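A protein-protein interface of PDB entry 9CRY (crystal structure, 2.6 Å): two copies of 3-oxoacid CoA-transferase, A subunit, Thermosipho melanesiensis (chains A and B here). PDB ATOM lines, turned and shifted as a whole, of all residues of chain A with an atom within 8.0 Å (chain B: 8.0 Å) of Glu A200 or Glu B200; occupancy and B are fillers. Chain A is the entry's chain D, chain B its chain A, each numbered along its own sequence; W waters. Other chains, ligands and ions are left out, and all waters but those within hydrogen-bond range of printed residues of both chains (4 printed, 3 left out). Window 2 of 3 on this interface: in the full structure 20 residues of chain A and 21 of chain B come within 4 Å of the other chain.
O of Asn B199 lies within hydrogen-bond range of NZ of Lys A202.
The backbone carbonyl oxygen (O) of Tyr B165 sits close to the side-chain amide oxygen (OD1) of Asn A199 (3.5 Å).
The side-chain amide oxygen (OD1) of Asn B199 lies close to the backbone carbonyl oxygen (O) of Tyr A165 (3.3 Å).
O of Asn A199 sits at hydrogen-bond distance from NZ of Lys B202.
The side-chain carboxylate (OE1) of Glu A170 lies within salt-bridge range of the side-chain amino group (NZ) of Lys A202.
The side-chain carboxylate (OE1) of Glu A200 is in hydrogen-bond range of the backbone NH (N) of Ser A197 (3.1 Å).
The backbone NH (N) of Ser B197 sits at hydrogen-bond distance from the side-chain carboxylate (OE1) of Glu B200.
The side-chain carboxylate (OE1) of Glu B170 lies within salt-bridge range of the side-chain amino group (NZ) of Lys B202.
The backbone NH (N) of Lys A202 sits at hydrogen-bond distance from the backbone carbonyl oxygen (O) of Leu A163.
The side-chain hydroxyl (OH) of Tyr B165 lies within hydrogen-bond range of the side-chain hydroxyl (OG1) of Thr B203 (2.7 Å).
OE2 of Glu A200 touches OE2 of Glu B200 (3.8 Å).
Of chain B, only Glu B200 (3.8 Å) comes within 4 Å of Glu A200.
Glu B200 touches just one residue of chain A: Glu A200.
Of the printed residues of chain A, Tyr B165 touches Asn A199 (3.5 Å).
Of the printed residues of chain B, Asn A199 touches Tyr B165 (3.5 Å) and Lys B202 (3.3 Å).
Of the printed residues of chain A, Lys B202 touches Asn A199 (3.3 Å).
Printed residues of chain B within 4 Å of Tyr A165: Asn B199 (3.3 Å).
Ser A197 touches none of the printed residues of chain B.
Of the 16 printed residues of chain B, 4 touch a printed residue of chain A.
Among the printed residues, 5 pairs touch across the chains.
Among the printed residues, no Asp or Glu carboxylate lies within 4 Å of a Lys or Arg side-chain nitrogen of the other chain.
Tyr A165 touches Asn B199, and with the chains exchanged Asn A199 touches Tyr B165.
Asn A199 touches Lys B202, and with the chains exchanged Lys A202 touches Asn B199.
Glu A200 touches its own counterpart, Glu B200.
16 positions are printed for both chains.
Water W1 lies within hydrogen-bond range of OD1 of Asn B199 (2.6 Å), NZ of Lys A202 (2.7 Å) and O of Tyr A165 (2.9 Å).
Water W4 lies within hydrogen-bond range of OE1 of Glu A170 (2.8 Å) and OD1 of Asn B199 (3.3 Å).
Water W3 lies within hydrogen-bond range of the backbone carbonyl oxygen (O) of Asn A199 and the backbone carbonyl oxygen (O) of Glu B200.
Water W2 bridges O of Asn B199 (3.3 Å) and O of Glu A200 (3.4 Å).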
ATOM      1  N   LYS A 156      23.813 -17.502  22.046  1.00  0.00           N
ATOM      2  CA  LYS A 156      24.415 -16.470  21.221  1.00  0.00           C
ATOM      3  C   LYS A 156      23.397 -15.376  20.949  1.00  0.00           C
ATOM      4  O   LYS A 156      22.192 -15.632  20.893  1.00  0.00           O
ATOM      5  CB  LYS A 156      24.874 -17.030  19.873  1.00  0.00           C
ATOM      6  CG  LYS A 156      26.037 -17.978  19.884  1.00  0.00           C
ATOM      7  CD  LYS A 156      26.190 -18.522  18.470  1.00  0.00           C
ATOM      8  CE  LYS A 156      27.348 -19.478  18.313  1.00  0.00           C
ATOM      9  NZ  LYS A 156      27.594 -19.743  16.856  1.00  0.00           N
ATOM     10  N   ASN A 162      19.210 -10.646  18.085  1.00  0.00           N
ATOM     11  CA  ASN A 162      18.653 -11.958  17.789  1.00  0.00           C
ATOM     12  C   ASN A 162      19.335 -13.009  18.646  1.00  0.00           C
ATOM     13  O   ASN A 162      20.558 -12.996  18.798  1.00  0.00           O
ATOM     14  CB  ASN A 162      18.873 -12.285  16.313  1.00  0.00           C
ATOM     15  CG  ASN A 162      18.083 -11.403  15.395  1.00  0.00           C
ATOM     16  OD1 ASN A 162      16.929 -11.110  15.652  1.00  0.00           O
ATOM     17  ND2 ASN A 162      18.717 -10.942  14.335  1.00  0.00           N
ATOM     18  N   LEU A 163      18.550 -13.953  19.161  1.00  0.00           N
ATOM     19  CA  LEU A 163      19.072 -15.023  20.000  1.00  0.00           C
ATOM     20  C   LEU A 163      18.858 -16.403  19.379  1.00  0.00           C
ATOM     21  O   LEU A 163      17.837 -16.656  18.736  1.00  0.00           O
ATOM     22  CB  LEU A 163      18.417 -14.984  21.376  1.00  0.00           C
ATOM     23  CG  LEU A 163      18.373 -13.661  22.131  1.00  0.00           C
ATOM     24  CD1 LEU A 163      17.549 -13.850  23.394  1.00  0.00           C
ATOM     25  CD2 LEU A 163      19.756 -13.214  22.446  1.00  0.00           C
ATOM     26  N   VAL A 164      19.834 -17.295  19.584  1.00  0.00           N
ATOM     27  CA  VAL A 164      19.646 -18.736  19.448  1.00  0.00           C
ATOM     28  C   VAL A 164      19.923 -19.392  20.796  1.00  0.00           C
ATOM     29  O   VAL A 164      20.680 -18.872  21.619  1.00  0.00           O
ATOM     30  CB  VAL A 164      20.572 -19.362  18.378  1.00  0.00           C
ATOM     31  CG1 VAL A 164      20.158 -18.961  16.978  1.00  0.00           C
ATOM     32  CG2 VAL A 164      22.005 -18.990  18.657  1.00  0.00           C
ATOM     33  N   TYR A 165      19.330 -20.558  21.005  1.00  0.00           N
ATOM     34  CA  TYR A 165      19.526 -21.384  22.186  1.00  0.00           C
ATOM     35  C   TYR A 165      20.278 -22.661  21.825  1.00  0.00           C
ATOM     36  O   TYR A 165      20.563 -22.937  20.662  1.00  0.00           O
ATOM     37  CB  TYR A 165      18.171 -21.674  22.824  1.00  0.00           C
ATOM     38  CG  TYR A 165      17.387 -20.413  23.059  1.00  0.00           C
ATOM     39  CD1 TYR A 165      17.578 -19.674  24.215  1.00  0.00           C
ATOM     40  CD2 TYR A 165      16.487 -19.930  22.114  1.00  0.00           C
ATOM     41  CE1 TYR A 165      16.869 -18.500  24.446  1.00  0.00           C
ATOM     42  CE2 TYR A 165      15.774 -18.758  22.331  1.00  0.00           C
ATOM     43  CZ  TYR A 165      15.975 -18.045  23.505  1.00  0.00           C
ATOM     44  OH  TYR A 165      15.290 -16.883  23.772  1.00  0.00           O
ATOM     45  N   GLU A 170      17.103 -24.566  26.082  1.00  0.00           N
ATOM     46  CA  GLU A 170      16.055 -23.715  25.526  1.00  0.00           C
ATOM     47  C   GLU A 170      14.888 -23.560  26.495  1.00  0.00           C
ATOM     48  O   GLU A 170      14.496 -22.437  26.828  1.00  0.00           O
ATOM     49  CB  GLU A 170      15.543 -24.260  24.185  1.00  0.00           C
ATOM     50  CG  GLU A 170      14.550 -23.303  23.506  1.00  0.00           C
ATOM     51  CD  GLU A 170      14.131 -23.699  22.085  1.00  0.00           C
ATOM     52  OE1 GLU A 170      14.701 -24.642  21.503  1.00  0.00           O
ATOM     53  OE2 GLU A 170      13.215 -23.063  21.532  1.00  0.00           O
ATOM     54  N   GLY A 194      24.323 -11.727  10.674  1.00  0.00           N
ATOM     55  CA  GLY A 194      24.536 -12.630   9.571  1.00  0.00           C
ATOM     56  C   GLY A 194      25.146 -13.946   9.993  1.00  0.00           C
ATOM     57  O   GLY A 194      25.257 -14.845   9.161  1.00  0.00           O
ATOM     58  N   THR A 195      25.583 -14.056  11.249  1.00  0.00           N
ATOM     59  CA  THR A 195      26.029 -15.315  11.838  1.00  0.00           C
ATOM     60  C   THR A 195      24.846 -16.201  12.214  1.00  0.00           C
ATOM     61  O   THR A 195      24.953 -17.425  12.173  1.00  0.00           O
ATOM     62  CB  THR A 195      26.881 -15.023  13.084  1.00  0.00           C
ATOM     63  OG1 THR A 195      28.097 -14.371  12.706  1.00  0.00           O
ATOM     64  CG2 THR A 195      27.219 -16.271  13.838  1.00  0.00           C
ATOM     65  N   LEU A 196      23.724 -15.601  12.591  1.00  0.00           N
ATOM     66  CA  LEU A 196      22.505 -16.319  12.927  1.00  0.00           C
ATOM     67  C   LEU A 196      21.563 -16.124  11.748  1.00  0.00           C
ATOM     68  O   LEU A 196      21.221 -14.988  11.406  1.00  0.00           O
ATOM     69  CB  LEU A 196      21.864 -15.806  14.220  1.00  0.00           C
ATOM     70  CG  LEU A 196      22.790 -15.561  15.420  1.00  0.00           C
ATOM     71  CD1 LEU A 196      22.046 -15.100  16.669  1.00  0.00           C
ATOM     72  CD2 LEU A 196      23.598 -16.857  15.654  1.00  0.00           C
ATOM     73  N   SER A 197      21.189 -17.212  11.115  1.00  0.00           N
ATOM     74  CA  SER A 197      20.398 -17.182   9.898  1.00  0.00           C
ATOM     75  C   SER A 197      18.944 -16.843  10.223  1.00  0.00           C
ATOM     76  O   SER A 197      18.468 -17.090  11.338  1.00  0.00           O
ATOM     77  CB  SER A 197      20.493 -18.532   9.190  1.00  0.00           C
ATOM     78  OG  SER A 197      19.301 -18.869   8.520  1.00  0.00           O
ATOM     79  N   PRO A 198      18.219 -16.261   9.271  1.00  0.00           N
ATOM     80  CA  PRO A 198      16.784 -16.049   9.504  1.00  0.00           C
ATOM     81  C   PRO A 198      16.047 -17.344   9.794  1.00  0.00           C
ATOM     82  O   PRO A 198      15.062 -17.322  10.535  1.00  0.00           O
ATOM     83  CB  PRO A 198      16.302 -15.388   8.203  1.00  0.00           C
ATOM     84  CG  PRO A 198      17.538 -14.884   7.547  1.00  0.00           C
ATOM     85  CD  PRO A 198      18.623 -15.849   7.921  1.00  0.00           C
ATOM     86  N   ASN A 199      16.481 -18.475   9.232  1.00  0.00           N
ATOM     87  CA  ASN A 199      15.789 -19.735   9.477  1.00  0.00           C
ATOM     88  C   ASN A 199      16.109 -20.314  10.862  1.00  0.00           C
ATOM     89  O   ASN A 199      15.374 -21.185  11.339  1.00  0.00           O
ATOM     90  CB  ASN A 199      16.134 -20.773   8.400  1.00  0.00           C
ATOM     91  CG  ASN A 199      15.541 -20.435   7.026  1.00  0.00           C
ATOM     92  OD1 ASN A 199      14.347 -20.193   6.859  1.00  0.00           O
ATOM     93  ND2 ASN A 199      16.387 -20.503   6.021  1.00  0.00           N
ATOM     94  N   GLU A 200      17.188 -19.867  11.508  1.00  0.00           N
ATOM     95  CA  GLU A 200      17.641 -20.451  12.761  1.00  0.00           C
ATOM     96  C   GLU A 200      17.250 -19.679  14.009  1.00  0.00           C
ATOM     97  O   GLU A 200      17.257 -20.250  15.107  1.00  0.00           O
ATOM     98  CB  GLU A 200      19.166 -20.496  12.835  1.00  0.00           C
ATOM     99  CG  GLU A 200      19.928 -21.109  11.731  1.00  0.00           C
ATOM    100  CD  GLU A 200      21.435 -20.891  11.942  1.00  0.00           C
ATOM    101  OE1 GLU A 200      21.782 -19.867  12.576  1.00  0.00           O
ATOM    102  OE2 GLU A 200      22.261 -21.733  11.513  1.00  0.00           O
ATOM    103  N   ILE A 201      17.034 -18.373  13.887  1.00  0.00           N
ATOM    104  CA  ILE A 201      16.879 -17.517  15.052  1.00  0.00           C
ATOM    105  C   ILE A 201      15.572 -17.874  15.737  1.00  0.00           C
ATOM    106  O   ILE A 201      14.535 -18.030  15.083  1.00  0.00           O
ATOM    107  CB  ILE A 201      16.895 -16.042  14.617  1.00  0.00           C
ATOM    108  CG1 ILE A 201      18.309 -15.599  14.261  1.00  0.00           C
ATOM    109  CG2 ILE A 201      16.383 -15.148  15.732  1.00  0.00           C
ATOM    110  CD1 ILE A 201      18.376 -14.347  13.409  1.00  0.00           C
ATOM    111  N   LYS A 202      15.598 -17.977  17.059  1.00  0.00           N
ATOM    112  CA  LYS A 202      14.382 -18.301  17.791  1.00  0.00           C
ATOM    113  C   LYS A 202      13.779 -17.143  18.581  1.00  0.00           C
ATOM    114  O   LYS A 202      12.572 -17.167  18.838  1.00  0.00           O
ATOM    115  CB  LYS A 202      14.641 -19.505  18.704  1.00  0.00           C
ATOM    116  CG  LYS A 202      14.815 -20.787  17.887  1.00  0.00           C
ATOM    117  CD  LYS A 202      15.092 -22.009  18.751  1.00  0.00           C
ATOM    118  CE  LYS A 202      15.066 -23.265  17.894  1.00  0.00           C
ATOM    119  NZ  LYS A 202      15.618 -24.467  18.592  1.00  0.00           N
ATOM    120  N   THR A 203      14.556 -16.129  18.955  1.00  0.00           N
ATOM    121  CA  THR A 203      13.991 -14.926  19.565  1.00  0.00           C
ATOM    122  C   THR A 203      14.507 -13.673  18.867  1.00  0.00           C
ATOM    123  O   THR A 203      15.734 -13.437  18.850  1.00  0.00           O
ATOM    124  CB  THR A 203      14.317 -14.888  21.055  1.00  0.00           C
ATOM    125  OG1 THR A 203      13.740 -16.029  21.704  1.00  0.00           O
ATOM    126  CG2 THR A 203      13.757 -13.636  21.681  1.00  0.00           C
ATOM    127  N   LYS B 156      13.325 -29.252   3.248  1.00  0.00           N
ATOM    128  CA  LYS B 156      14.100 -30.479   3.335  1.00  0.00           C
ATOM    129  C   LYS B 156      13.553 -31.405   4.428  1.00  0.00           C
ATOM    130  O   LYS B 156      13.026 -30.959   5.457  1.00  0.00           O
ATOM    131  CB  LYS B 156      15.562 -30.205   3.709  1.00  0.00           C
ATOM    132  CG  LYS B 156      16.229 -29.089   2.963  1.00  0.00           C
ATOM    133  CD  LYS B 156      17.527 -28.815   3.661  1.00  0.00           C
ATOM    134  CE  LYS B 156      18.621 -28.345   2.702  1.00  0.00           C
ATOM    135  NZ  LYS B 156      18.888 -26.941   3.055  1.00  0.00           N
ATOM    136  N   ASN B 162      12.546 -35.537   9.872  1.00  0.00           N
ATOM    137  CA  ASN B 162      12.702 -34.193  10.414  1.00  0.00           C
ATOM    138  C   ASN B 162      12.640 -33.150   9.304  1.00  0.00           C
ATOM    139  O   ASN B 162      13.232 -33.328   8.239  1.00  0.00           O
ATOM    140  CB  ASN B 162      14.047 -34.081  11.127  1.00  0.00           C
ATOM    141  CG  ASN B 162      14.125 -34.904  12.384  1.00  0.00           C
ATOM    142  OD1 ASN B 162      13.220 -34.885  13.214  1.00  0.00           O
ATOM    143  ND2 ASN B 162      15.202 -35.661  12.518  1.00  0.00           N
ATOM    144  N   LEU B 163      11.964 -32.033   9.569  1.00  0.00           N
ATOM    145  CA  LEU B 163      11.721 -31.010   8.557  1.00  0.00           C
ATOM    146  C   LEU B 163      12.332 -29.670   8.958  1.00  0.00           C
ATOM    147  O   LEU B 163      12.342 -29.298  10.138  1.00  0.00           O
ATOM    148  CB  LEU B 163      10.217 -30.836   8.314  1.00  0.00           C
ATOM    149  CG  LEU B 163       9.408 -32.061   7.881  1.00  0.00           C
ATOM    150  CD1 LEU B 163       7.965 -31.621   7.745  1.00  0.00           C
ATOM    151  CD2 LEU B 163       9.927 -32.629   6.588  1.00  0.00           C
ATOM    152  N   VAL B 164      12.851 -28.952   7.959  1.00  0.00           N
ATOM    153  CA  VAL B 164      13.092 -27.521   8.063  1.00  0.00           C
ATOM    154  C   VAL B 164      12.367 -26.805   6.931  1.00  0.00           C
ATOM    155  O   VAL B 164      12.109 -27.360   5.856  1.00  0.00           O
ATOM    156  CB  VAL B 164      14.593 -27.165   8.023  1.00  0.00           C
ATOM    157  CG1 VAL B 164      15.329 -27.791   9.177  1.00  0.00           C
ATOM    158  CG2 VAL B 164      15.184 -27.557   6.708  1.00  0.00           C
ATOM    159  N   TYR B 165      12.040 -25.551   7.197  1.00  0.00           N
ATOM    160  CA  TYR B 165      11.344 -24.669   6.285  1.00  0.00           C
ATOM    161  C   TYR B 165      12.293 -23.584   5.789  1.00  0.00           C
ATOM    162  O   TYR B 165      13.449 -23.489   6.215  1.00  0.00           O
ATOM    163  CB  TYR B 165      10.121 -24.096   7.002  1.00  0.00           C
ATOM    164  CG  TYR B 165       9.197 -25.164   7.538  1.00  0.00           C
ATOM    165  CD1 TYR B 165       8.257 -25.769   6.720  1.00  0.00           C
ATOM    166  CD2 TYR B 165       9.309 -25.612   8.854  1.00  0.00           C
ATOM    167  CE1 TYR B 165       7.414 -26.755   7.205  1.00  0.00           C
ATOM    168  CE2 TYR B 165       8.480 -26.612   9.341  1.00  0.00           C
ATOM    169  CZ  TYR B 165       7.533 -27.173   8.508  1.00  0.00           C
ATOM    170  OH  TYR B 165       6.708 -28.151   8.973  1.00  0.00           O
ATOM    171  N   GLU B 170       7.422 -20.884   5.518  1.00  0.00           N
ATOM    172  CA  GLU B 170       7.019 -21.582   6.731  1.00  0.00           C
ATOM    173  C   GLU B 170       5.527 -21.409   6.972  1.00  0.00           C
ATOM    174  O   GLU B 170       4.772 -22.384   7.034  1.00  0.00           O
ATOM    175  CB  GLU B 170       7.804 -21.077   7.945  1.00  0.00           C
ATOM    176  CG  GLU B 170       7.539 -21.827   9.243  1.00  0.00           C
ATOM    177  CD  GLU B 170       8.559 -21.478  10.320  1.00  0.00           C
ATOM    178  OE1 GLU B 170       9.517 -20.712  10.050  1.00  0.00           O
ATOM    179  OE2 GLU B 170       8.431 -21.999  11.443  1.00  0.00           O
ATOM    180  N   GLY B 194      21.625 -35.996  10.314  1.00  0.00           N
ATOM    181  CA  GLY B 194      22.776 -35.255  10.761  1.00  0.00           C
ATOM    182  C   GLY B 194      23.025 -34.009   9.949  1.00  0.00           C
ATOM    183  O   GLY B 194      23.870 -33.194  10.330  1.00  0.00           O
ATOM    184  N   THR B 195      22.305 -33.837   8.840  1.00  0.00           N
ATOM    185  CA  THR B 195      22.390 -32.587   8.099  1.00  0.00           C
ATOM    186  C   THR B 195      21.585 -31.487   8.789  1.00  0.00           C
ATOM    187  O   THR B 195      21.975 -30.313   8.769  1.00  0.00           O
ATOM    188  CB  THR B 195      21.873 -32.779   6.668  1.00  0.00           C
ATOM    189  OG1 THR B 195      22.721 -33.664   5.928  1.00  0.00           O
ATOM    190  CG2 THR B 195      21.808 -31.454   5.970  1.00  0.00           C
ATOM    191  N   LEU B 196      20.446 -31.840   9.366  1.00  0.00           N
ATOM    192  CA  LEU B 196      19.595 -30.895  10.078  1.00  0.00           C
ATOM    193  C   LEU B 196      19.904 -31.040  11.557  1.00  0.00           C
ATOM    194  O   LEU B 196      19.774 -32.129  12.117  1.00  0.00           O
ATOM    195  CB  LEU B 196      18.114 -31.140   9.808  1.00  0.00           C
ATOM    196  CG  LEU B 196      17.794 -31.280   8.328  1.00  0.00           C
ATOM    197  CD1 LEU B 196      16.361 -31.760   8.130  1.00  0.00           C
ATOM    198  CD2 LEU B 196      18.013 -29.961   7.553  1.00  0.00           C
ATOM    199  N   SER B 197      20.331 -29.951  12.167  1.00  0.00           N
ATOM    200  CA  SER B 197      20.761 -29.949  13.544  1.00  0.00           C
ATOM    201  C   SER B 197      19.569 -30.087  14.486  1.00  0.00           C
ATOM    202  O   SER B 197      18.431 -29.773  14.129  1.00  0.00           O
ATOM    203  CB  SER B 197      21.527 -28.659  13.829  1.00  0.00           C
ATOM    204  OG  SER B 197      21.378 -28.264  15.176  1.00  0.00           O
ATOM    205  N   PRO B 198      19.807 -30.580  15.700  1.00  0.00           N
ATOM    206  CA  PRO B 198      18.736 -30.543  16.704  1.00  0.00           C
ATOM    207  C   PRO B 198      18.221 -29.127  16.943  1.00  0.00           C
ATOM    208  O   PRO B 198      17.051 -28.954  17.288  1.00  0.00           O
ATOM    209  CB  PRO B 198      19.401 -31.134  17.954  1.00  0.00           C
ATOM    210  CG  PRO B 198      20.491 -31.971  17.441  1.00  0.00           C
ATOM    211  CD  PRO B 198      20.953 -31.397  16.132  1.00  0.00           C
ATOM    212  N   ASN B 199      19.073 -28.114  16.822  1.00  0.00           N
ATOM    213  CA  ASN B 199      18.704 -26.722  17.059  1.00  0.00           C
ATOM    214  C   ASN B 199      18.022 -26.063  15.862  1.00  0.00           C
ATOM    215  O   ASN B 199      17.420 -25.000  16.028  1.00  0.00           O
ATOM    216  CB  ASN B 199      19.979 -25.979  17.454  1.00  0.00           C
ATOM    217  CG  ASN B 199      20.329 -26.142  18.937  1.00  0.00           C
ATOM    218  OD1 ASN B 199      19.491 -25.951  19.826  1.00  0.00           O
ATOM    219  ND2 ASN B 199      21.565 -26.543  19.201  1.00  0.00           N
ATOM    220  N   GLU B 200      18.073 -26.674  14.678  1.00  0.00           N
ATOM    221  CA  GLU B 200      17.425 -26.108  13.502  1.00  0.00           C
ATOM    222  C   GLU B 200      16.095 -26.746  13.156  1.00  0.00           C
ATOM    223  O   GLU B 200      15.308 -26.130  12.436  1.00  0.00           O
ATOM    224  CB  GLU B 200      18.291 -26.242  12.243  1.00  0.00           C
ATOM    225  CG  GLU B 200      19.672 -25.682  12.284  1.00  0.00           C
ATOM    226  CD  GLU B 200      20.490 -26.084  11.045  1.00  0.00           C
ATOM    227  OE1 GLU B 200      20.164 -27.097  10.373  1.00  0.00           O
ATOM    228  OE2 GLU B 200      21.456 -25.361  10.725  1.00  0.00           O
ATOM    229  N   ILE B 201      15.860 -27.994  13.551  1.00  0.00           N
ATOM    230  CA  ILE B 201      14.679 -28.704  13.075  1.00  0.00           C
ATOM    231  C   ILE B 201      13.458 -28.017  13.658  1.00  0.00           C
ATOM    232  O   ILE B 201      13.454 -27.613  14.829  1.00  0.00           O
ATOM    233  CB  ILE B 201      14.744 -30.191  13.469  1.00  0.00           C
ATOM    234  CG1 ILE B 201      15.766 -30.918  12.591  1.00  0.00           C
ATOM    235  CG2 ILE B 201      13.372 -30.852  13.347  1.00  0.00           C
ATOM    236  CD1 ILE B 201      16.359 -32.147  13.242  1.00  0.00           C
ATOM    237  N   LYS B 202      12.428 -27.838  12.835  1.00  0.00           N
ATOM    238  CA  LYS B 202      11.188 -27.242  13.306  1.00  0.00           C
ATOM    239  C   LYS B 202      10.008 -28.198  13.392  1.00  0.00           C
ATOM    240  O   LYS B 202       9.080 -27.922  14.154  1.00  0.00           O
ATOM    241  CB  LYS B 202      10.797 -26.051  12.421  1.00  0.00           C
ATOM    242  CG  LYS B 202      11.836 -24.934  12.511  1.00  0.00           C
ATOM    243  CD  LYS B 202      11.378 -23.595  11.920  1.00  0.00           C
ATOM    244  CE  LYS B 202      12.399 -22.491  12.177  1.00  0.00           C
ATOM    245  NZ  LYS B 202      12.048 -21.276  11.384  1.00  0.00           N
ATOM    246  N   THR B 203       9.998 -29.277  12.613  1.00  0.00           N
ATOM    247  CA  THR B 203       8.968 -30.313  12.708  1.00  0.00           C
ATOM    248  C   THR B 203       9.643 -31.671  12.862  1.00  0.00           C
ATOM    249  O   THR B 203      10.406 -32.085  11.965  1.00  0.00           O
ATOM    250  CB  THR B 203       8.055 -30.282  11.482  1.00  0.00           C
ATOM    251  OG1 THR B 203       7.369 -29.029  11.430  1.00  0.00           O
ATOM    252  CG2 THR B 203       7.025 -31.396  11.538  1.00  0.00           C
HETATM  253  O   HOH W   1      18.024 -23.826  19.666  1.00  0.00           O
HETATM  254  O   HOH W   2      18.258 -22.284  17.607  1.00  0.00           O
HETATM  255  O   HOH W   3      15.567 -23.913  10.303  1.00  0.00           O
HETATM  256  O   HOH W   4      16.884 -26.318  21.744  1.00  0.00           O
